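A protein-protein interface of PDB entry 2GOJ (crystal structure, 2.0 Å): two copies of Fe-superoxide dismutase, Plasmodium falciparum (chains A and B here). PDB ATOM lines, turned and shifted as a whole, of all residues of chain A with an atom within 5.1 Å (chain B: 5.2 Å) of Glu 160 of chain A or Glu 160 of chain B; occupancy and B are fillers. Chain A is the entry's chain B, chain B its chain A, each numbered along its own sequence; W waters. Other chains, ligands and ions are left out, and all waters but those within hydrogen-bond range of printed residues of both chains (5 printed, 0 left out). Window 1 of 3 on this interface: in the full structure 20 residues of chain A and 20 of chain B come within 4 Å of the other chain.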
ATOM      1  N   HIS A  30     -34.814 -12.206  31.885  1.00  0.00           N
ATOM      2  CA  HIS A  30     -35.243 -13.163  30.865  1.00  0.00           C
ATOM      3  C   HIS A  30     -36.170 -14.206  31.468  1.00  0.00           C
ATOM      4  O   HIS A  30     -37.307 -14.335  31.056  1.00  0.00           O
ATOM      5  CB  HIS A  30     -34.045 -13.857  30.199  1.00  0.00           C
ATOM      6  CG  HIS A  30     -33.236 -12.956  29.325  1.00  0.00           C
ATOM      7  ND1 HIS A  30     -33.579 -12.681  28.019  1.00  0.00           N
ATOM      8  CD2 HIS A  30     -32.105 -12.254  29.574  1.00  0.00           C
ATOM      9  CE1 HIS A  30     -32.681 -11.863  27.494  1.00  0.00           C
ATOM     10  NE2 HIS A  30     -31.777 -11.586  28.417  1.00  0.00           N
ATOM     11  N   SER A 120     -30.375 -19.757  18.295  1.00  0.00           N
ATOM     12  CA  SER A 120     -30.691 -19.900  19.706  1.00  0.00           C
ATOM     13  C   SER A 120     -31.047 -21.347  20.005  1.00  0.00           C
ATOM     14  O   SER A 120     -31.647 -22.033  19.169  1.00  0.00           O
ATOM     15  CB  SER A 120     -31.866 -18.990  20.087  1.00  0.00           C
ATOM     16  OG  SER A 120     -31.604 -17.610  19.803  1.00  0.00           O
ATOM     17  N   ILE A 158     -27.450 -22.141  25.165  1.00  0.00           N
ATOM     18  CA  ILE A 158     -26.511 -21.483  24.253  1.00  0.00           C
ATOM     19  C   ILE A 158     -27.159 -20.328  23.463  1.00  0.00           C
ATOM     20  O   ILE A 158     -26.574 -19.838  22.505  1.00  0.00           O
ATOM     21  CB  ILE A 158     -25.733 -22.482  23.323  1.00  0.00           C
ATOM     22  CG1 ILE A 158     -26.661 -23.468  22.602  1.00  0.00           C
ATOM     23  CG2 ILE A 158     -24.643 -23.239  24.110  1.00  0.00           C
ATOM     24  CD1 ILE A 158     -27.312 -22.884  21.386  1.00  0.00           C
ATOM     25  N   TRP A 159     -28.341 -19.873  23.886  1.00  0.00           N
ATOM     26  CA  TRP A 159     -28.818 -18.542  23.499  1.00  0.00           C
ATOM     27  C   TRP A 159     -27.714 -17.549  23.814  1.00  0.00           C
ATOM     28  O   TRP A 159     -26.999 -17.702  24.812  1.00  0.00           O
ATOM     29  CB  TRP A 159     -30.046 -18.109  24.284  1.00  0.00           C
ATOM     30  CG  TRP A 159     -31.339 -18.767  23.880  1.00  0.00           C
ATOM     31  CD1 TRP A 159     -31.655 -20.097  23.955  1.00  0.00           C
ATOM     32  CD2 TRP A 159     -32.505 -18.107  23.392  1.00  0.00           C
ATOM     33  NE1 TRP A 159     -32.942 -20.301  23.524  1.00  0.00           N
ATOM     34  CE2 TRP A 159     -33.490 -19.098  23.172  1.00  0.00           C
ATOM     35  CE3 TRP A 159     -32.811 -16.777  23.079  1.00  0.00           C
ATOM     36  CZ2 TRP A 159     -34.752 -18.798  22.657  1.00  0.00           C
ATOM     37  CZ3 TRP A 159     -34.065 -16.480  22.586  1.00  0.00           C
ATOM     38  CH2 TRP A 159     -35.025 -17.483  22.382  1.00  0.00           C
ATOM     39  N   GLU A 160     -27.587 -16.522  22.986  1.00  0.00           N
ATOM     40  CA  GLU A 160     -26.490 -15.582  23.138  1.00  0.00           C
ATOM     41  C   GLU A 160     -26.544 -14.814  24.456  1.00  0.00           C
ATOM     42  O   GLU A 160     -25.495 -14.488  24.998  1.00  0.00           O
ATOM     43  CB  GLU A 160     -26.388 -14.644  21.935  1.00  0.00           C
ATOM     44  CG  GLU A 160     -26.031 -15.341  20.634  1.00  0.00           C
ATOM     45  CD  GLU A 160     -25.993 -14.397  19.437  1.00  0.00           C
ATOM     46  OE1 GLU A 160     -26.920 -13.569  19.276  1.00  0.00           O
ATOM     47  OE2 GLU A 160     -25.044 -14.504  18.636  1.00  0.00           O
ATOM     48  N   HIS A 161     -27.731 -14.568  25.012  1.00  0.00           N
ATOM     49  CA  HIS A 161     -27.819 -13.839  26.283  1.00  0.00           C
ATOM     50  C   HIS A 161     -27.167 -14.612  27.440  1.00  0.00           C
ATOM     51  O   HIS A 161     -26.790 -14.011  28.433  1.00  0.00           O
ATOM     52  CB  HIS A 161     -29.267 -13.450  26.643  1.00  0.00           C
ATOM     53  CG  HIS A 161     -30.189 -14.618  26.806  1.00  0.00           C
ATOM     54  ND1 HIS A 161     -31.228 -14.872  25.937  1.00  0.00           N
ATOM     55  CD2 HIS A 161     -30.228 -15.602  27.734  1.00  0.00           C
ATOM     56  CE1 HIS A 161     -31.862 -15.966  26.317  1.00  0.00           C
ATOM     57  NE2 HIS A 161     -31.273 -16.433  27.402  1.00  0.00           N
ATOM     58  N   ALA A 162     -27.064 -15.938  27.309  1.00  0.00           N
ATOM     59  CA  ALA A 162     -26.441 -16.800  28.325  1.00  0.00           C
ATOM     60  C   ALA A 162     -24.976 -16.472  28.574  1.00  0.00           C
ATOM     61  O   ALA A 162     -24.463 -16.698  29.669  1.00  0.00           O
ATOM     62  CB  ALA A 162     -26.568 -18.258  27.933  1.00  0.00           C
ATOM     63  N   TYR A 163     -24.327 -15.919  27.553  1.00  0.00           N
ATOM     64  CA  TYR A 163     -22.883 -15.716  27.559  1.00  0.00           C
ATOM     65  C   TYR A 163     -22.382 -14.380  27.020  1.00  0.00           C
ATOM     66  O   TYR A 163     -21.216 -14.049  27.234  1.00  0.00           O
ATOM     67  CB  TYR A 163     -22.189 -16.880  26.824  1.00  0.00           C
ATOM     68  CG  TYR A 163     -22.524 -17.069  25.343  1.00  0.00           C
ATOM     69  CD1 TYR A 163     -21.862 -16.345  24.360  1.00  0.00           C
ATOM     70  CD2 TYR A 163     -23.447 -18.033  24.933  1.00  0.00           C
ATOM     71  CE1 TYR A 163     -22.142 -16.542  22.997  1.00  0.00           C
ATOM     72  CE2 TYR A 163     -23.732 -18.245  23.567  1.00  0.00           C
ATOM     73  CZ  TYR A 163     -23.081 -17.493  22.615  1.00  0.00           C
ATOM     74  OH  TYR A 163     -23.344 -17.693  21.275  1.00  0.00           O
ATOM     75  N   TYR A 164     -23.222 -13.592  26.353  1.00  0.00           N
ATOM     76  CA  TYR A 164     -22.688 -12.446  25.611  1.00  0.00           C
ATOM     77  C   TYR A 164     -22.006 -11.405  26.519  1.00  0.00           C
ATOM     78  O   TYR A 164     -21.055 -10.756  26.102  1.00  0.00           O
ATOM     79  CB  TYR A 164     -23.745 -11.786  24.684  1.00  0.00           C
ATOM     80  CG  TYR A 164     -23.123 -11.337  23.393  1.00  0.00           C
ATOM     81  CD1 TYR A 164     -22.763 -12.266  22.415  1.00  0.00           C
ATOM     82  CD2 TYR A 164     -22.825  -9.989  23.163  1.00  0.00           C
ATOM     83  CE1 TYR A 164     -22.128 -11.869  21.249  1.00  0.00           C
ATOM     84  CE2 TYR A 164     -22.198  -9.586  21.987  1.00  0.00           C
ATOM     85  CZ  TYR A 164     -21.855 -10.531  21.037  1.00  0.00           C
ATOM     86  OH  TYR A 164     -21.236 -10.153  19.870  1.00  0.00           O
ATOM     87  N   HIS B  30     -18.464 -11.481  14.139  1.00  0.00           N
ATOM     88  CA  HIS B  30     -19.575 -12.306  13.646  1.00  0.00           C
ATOM     89  C   HIS B  30     -19.578 -12.376  12.117  1.00  0.00           C
ATOM     90  O   HIS B  30     -19.530 -13.459  11.527  1.00  0.00           O
ATOM     91  CB  HIS B  30     -20.936 -11.779  14.135  1.00  0.00           C
ATOM     92  CG  HIS B  30     -21.169 -11.972  15.596  1.00  0.00           C
ATOM     93  ND1 HIS B  30     -21.605 -13.167  16.128  1.00  0.00           N
ATOM     94  CD2 HIS B  30     -21.005 -11.129  16.644  1.00  0.00           C
ATOM     95  CE1 HIS B  30     -21.705 -13.050  17.440  1.00  0.00           C
ATOM     96  NE2 HIS B  30     -21.355 -11.822  17.779  1.00  0.00           N
ATOM     97  N   SER B 120     -33.608 -15.950  17.420  1.00  0.00           N
ATOM     98  CA  SER B 120     -32.742 -15.194  16.518  1.00  0.00           C
ATOM     99  C   SER B 120     -33.440 -14.984  15.197  1.00  0.00           C
ATOM    100  O   SER B 120     -34.242 -15.812  14.791  1.00  0.00           O
ATOM    101  CB  SER B 120     -31.457 -15.969  16.250  1.00  0.00           C
ATOM    102  OG  SER B 120     -30.754 -16.236  17.444  1.00  0.00           O
ATOM    103  N   ILE B 158     -32.172  -8.809  14.627  1.00  0.00           N
ATOM    104  CA  ILE B 158     -32.614  -8.938  16.022  1.00  0.00           C
ATOM    105  C   ILE B 158     -32.064 -10.205  16.734  1.00  0.00           C
ATOM    106  O   ILE B 158     -32.546 -10.603  17.792  1.00  0.00           O
ATOM    107  CB  ILE B 158     -34.155  -8.796  16.144  1.00  0.00           C
ATOM    108  CG1 ILE B 158     -34.898  -9.763  15.223  1.00  0.00           C
ATOM    109  CG2 ILE B 158     -34.604  -7.367  15.814  1.00  0.00           C
ATOM    110  CD1 ILE B 158     -35.080 -11.074  15.793  1.00  0.00           C
ATOM    111  N   TRP B 159     -31.033 -10.824  16.165  1.00  0.00           N
ATOM    112  CA  TRP B 159     -30.182 -11.725  16.939  1.00  0.00           C
ATOM    113  C   TRP B 159     -29.703 -10.918  18.140  1.00  0.00           C
ATOM    114  O   TRP B 159     -29.442  -9.727  18.019  1.00  0.00           O
ATOM    115  CB  TRP B 159     -28.957 -12.159  16.134  1.00  0.00           C
ATOM    116  CG  TRP B 159     -29.188 -13.211  15.083  1.00  0.00           C
ATOM    117  CD1 TRP B 159     -29.981 -13.112  13.966  1.00  0.00           C
ATOM    118  CD2 TRP B 159     -28.577 -14.498  15.028  1.00  0.00           C
ATOM    119  NE1 TRP B 159     -29.901 -14.269  13.234  1.00  0.00           N
ATOM    120  CE2 TRP B 159     -29.051 -15.139  13.869  1.00  0.00           C
ATOM    121  CE3 TRP B 159     -27.678 -15.187  15.860  1.00  0.00           C
ATOM    122  CZ2 TRP B 159     -28.658 -16.434  13.511  1.00  0.00           C
ATOM    123  CZ3 TRP B 159     -27.289 -16.477  15.511  1.00  0.00           C
ATOM    124  CH2 TRP B 159     -27.776 -17.083  14.337  1.00  0.00           C
ATOM    125  N   GLU B 160     -29.587 -11.561  19.293  1.00  0.00           N
ATOM    126  CA  GLU B 160     -29.192 -10.856  20.525  1.00  0.00           C
ATOM    127  C   GLU B 160     -27.851 -10.120  20.439  1.00  0.00           C
ATOM    128  O   GLU B 160     -27.701  -9.071  21.032  1.00  0.00           O
ATOM    129  CB  GLU B 160     -29.250 -11.795  21.733  1.00  0.00           C
ATOM    130  CG  GLU B 160     -30.655 -12.301  21.998  1.00  0.00           C
ATOM    131  CD  GLU B 160     -30.758 -13.297  23.144  1.00  0.00           C
ATOM    132  OE1 GLU B 160     -29.934 -14.259  23.211  1.00  0.00           O
ATOM    133  OE2 GLU B 160     -31.707 -13.127  23.959  1.00  0.00           O
ATOM    134  N   HIS B 161     -26.915 -10.635  19.659  1.00  0.00           N
ATOM    135  CA  HIS B 161     -25.598 -10.007  19.499  1.00  0.00           C
ATOM    136  C   HIS B 161     -25.662  -8.621  18.848  1.00  0.00           C
ATOM    137  O   HIS B 161     -24.759  -7.819  19.027  1.00  0.00           O
ATOM    138  CB  HIS B 161     -24.618 -10.916  18.733  1.00  0.00           C
ATOM    139  CG  HIS B 161     -24.998 -11.192  17.308  1.00  0.00           C
ATOM    140  ND1 HIS B 161     -25.168 -12.472  16.822  1.00  0.00           N
ATOM    141  CD2 HIS B 161     -25.191 -10.361  16.253  1.00  0.00           C
ATOM    142  CE1 HIS B 161     -25.457 -12.413  15.532  1.00  0.00           C
ATOM    143  NE2 HIS B 161     -25.499 -11.144  15.170  1.00  0.00           N
ATOM    144  N   ALA B 162     -26.739  -8.350  18.115  1.00  0.00           N
ATOM    145  CA  ALA B 162     -26.941  -7.042  17.497  1.00  0.00           C
ATOM    146  C   ALA B 162     -27.117  -5.925  18.526  1.00  0.00           C
ATOM    147  O   ALA B 162     -26.800  -4.764  18.242  1.00  0.00           O
ATOM    148  CB  ALA B 162     -28.113  -7.082  16.572  1.00  0.00           C
ATOM    149  N   TYR B 163     -27.608  -6.263  19.713  1.00  0.00           N
ATOM    150  CA  TYR B 163     -27.927  -5.256  20.701  1.00  0.00           C
ATOM    151  C   TYR B 163     -27.478  -5.518  22.140  1.00  0.00           C
ATOM    152  O   TYR B 163     -27.525  -4.601  22.955  1.00  0.00           O
ATOM    153  CB  TYR B 163     -29.438  -4.992  20.660  1.00  0.00           C
ATOM    154  CG  TYR B 163     -30.341  -6.192  20.934  1.00  0.00           C
ATOM    155  CD1 TYR B 163     -30.676  -6.560  22.239  1.00  0.00           C
ATOM    156  CD2 TYR B 163     -30.878  -6.933  19.893  1.00  0.00           C
ATOM    157  CE1 TYR B 163     -31.516  -7.637  22.494  1.00  0.00           C
ATOM    158  CE2 TYR B 163     -31.726  -8.020  20.135  1.00  0.00           C
ATOM    159  CZ  TYR B 163     -32.047  -8.357  21.434  1.00  0.00           C
ATOM    160  OH  TYR B 163     -32.892  -9.424  21.673  1.00  0.00           O
ATOM    161  N   TYR B 164     -27.025  -6.723  22.475  1.00  0.00           N
ATOM    162  CA  TYR B 164     -26.900  -7.078  23.897  1.00  0.00           C
ATOM    163  C   TYR B 164     -25.866  -6.242  24.666  1.00  0.00           C
ATOM    164  O   TYR B 164     -26.035  -6.000  25.864  1.00  0.00           O
ATOM    165  CB  TYR B 164     -26.626  -8.578  24.107  1.00  0.00           C
ATOM    166  CG  TYR B 164     -27.342  -9.105  25.339  1.00  0.00           C
ATOM    167  CD1 TYR B 164     -28.705  -9.411  25.296  1.00  0.00           C
ATOM    168  CD2 TYR B 164     -26.671  -9.259  26.544  1.00  0.00           C
ATOM    169  CE1 TYR B 164     -29.380  -9.869  26.419  1.00  0.00           C
ATOM    170  CE2 TYR B 164     -27.330  -9.727  27.678  1.00  0.00           C
ATOM    171  CZ  TYR B 164     -28.677 -10.030  27.611  1.00  0.00           C
ATOM    172  OH  TYR B 164     -29.315 -10.476  28.730  1.00  0.00           O
HETATM  173  O   HOH W   1     -29.816 -16.116  21.201  1.00  0.00           O
HETATM  174  O   HOH W   2     -21.991  -7.785  18.234  1.00  0.00           O
HETATM  175  O   HOH W   3     -29.485 -14.500  19.000  1.00  0.00           O
HETATM  176  O   HOH W   4     -28.480 -12.538  30.330  1.00  0.00           O
HETATM  177  O   HOH W   5     -32.933 -18.906  16.999  1.00  0.00           O
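Of the 9 printed residues of chain B, 6 touch a printed residue of chain A.
Hydrophobic or aromatic side chains of chain B that line the printed part of chain A: His 30, Trp 159, His 161 and Tyr 164.
Of the 9 printed residues of chain A, 6 touch a printed residue of chain B.
Printed residues of chain A that touch a printed residue of chain B: His 30, Ser 120, Trp 159, Glu 160, His 161 and Tyr 164.
Hydrophobic or aromatic side chains of chain A that line the printed part of chain B: His 30, Trp 159, His 161 and Tyr 164.
Among the printed residues, no Asp or Glu carboxylate lies within 4 Å of a Lys or Arg side-chain nitrogen of the other chain.
Of chain B, only His 30 (3.8 Å), Trp 159 (3.9 Å), Glu 160 (3.3 Å) and His 161 (2.7 Å) come within 4 Å of Glu 160 of chain A.
Of the printed residues of chain B, Tyr 164 of chain A touches His 30 and His 161.
Of the printed residues of chain A, His 161 of chain B touches Glu 160 (2.7 Å) and Tyr 164 (3.6 Å).
Printed residues of chain B within 4 Å of His 30 of chain A: Glu 160 and Tyr 164.
Of the printed residues of chain B, Trp 159 of chain A touches Glu 160 (3.8 Å).
Of the printed residues of chain A, Tyr 164 of chain B touches His 30 and His 161.
The nearest residue of chain B that does not touch Glu 160 of chain A is Ser 120 of chain B (5.0 Å).
The nearest printed residue of chain A that does not touch Glu 160 of chain B is Ser 120 of chain A (5.1 Å).
Among the printed residues, merely in contact across the chains: His 161 of chain A with Tyr 164 of chain B (3.6 Å), Tyr 164 of chain A with His 161 of chain B (3.6 Å), Trp 159 of chain A with Glu 160 of chain B (3.8 Å), Glu 160 of chain A with His 30 of chain B (3.8 Å), Glu 160 of chain A with Trp 159 of chain B (3.9 Å) and His 30 of chain A with Glu 160 of chain B (3.9 Å).
The side-chain hydroxyl (OH) of Tyr 164 of chain A sits at hydrogen-bond distance from a ring nitrogen (NE2) of His 30 of chain B (2.7 Å).
OG of Ser 120 of chain B sits at hydrogen-bond distance from OG of Ser 120 of chain A (2.9 Å).
The side-chain carboxylate (OE1) of Glu 160 of chain B sits at hydrogen-bond distance from the backbone NH (N) of Glu 160 of chain A (3.3 Å).
The side-chain carboxylate (OE2) of Glu 160 of chain B lies within hydrogen-bond range of a ring nitrogen (ND1) of His 161 of chain A (2.7 Å).
The side-chain carboxylate (OE2) of Glu 160 of chain A is in hydrogen-bond range of a ring nitrogen (ND1) of His 161 of chain B.
A ring nitrogen (NE2) of His 30 of chain A lies within hydrogen-bond range of the side-chain hydroxyl (OH) of Tyr 164 of chain B, 2.7 Å away.
His 30 of chain A touches Tyr 164 of chain B, and with the chains exchanged Tyr 164 of chain A touches His 30 of chain B.
Trp 159 of chain A touches Glu 160 of chain B, and with the chains exchanged Glu 160 of chain A touches Trp 159 of chain B.
Glu 160 of chain B touches its own counterpart, Glu 160 of chain A.
Glu 160 of chain A touches His 161 of chain B, and with the chains exchanged His 161 of chain A touches Glu 160 of chain B.
Of the 12 pairs that touch across the chains among the printed residues, 12 have their exchanged pair printed and touching as well.
Water W3 lies within hydrogen-bond range of OG of Ser 120 of chain B, OE1 of Glu 160 of chain A and N of Glu 160 of chain B.
Water W1 lies within hydrogen-bond range of OG of Ser 120 of chain A (2.7 Å), OE1 of Glu 160 of chain B (2.7 Å) and N of Glu 160 of chain A (2.9 Å).
Water W4 lies within hydrogen-bond range of OH of Tyr 164 of chain B (2.7 Å) and O of His 161 of chain A (2.9 Å).
Water W2 bridges O of His 161 of chain B (2.9 Å) and OH of Tyr 164 of chain A (3.0 Å).
Water W5 bridges N of Ser 120 of chain A and N of Ser 120 of chain B.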
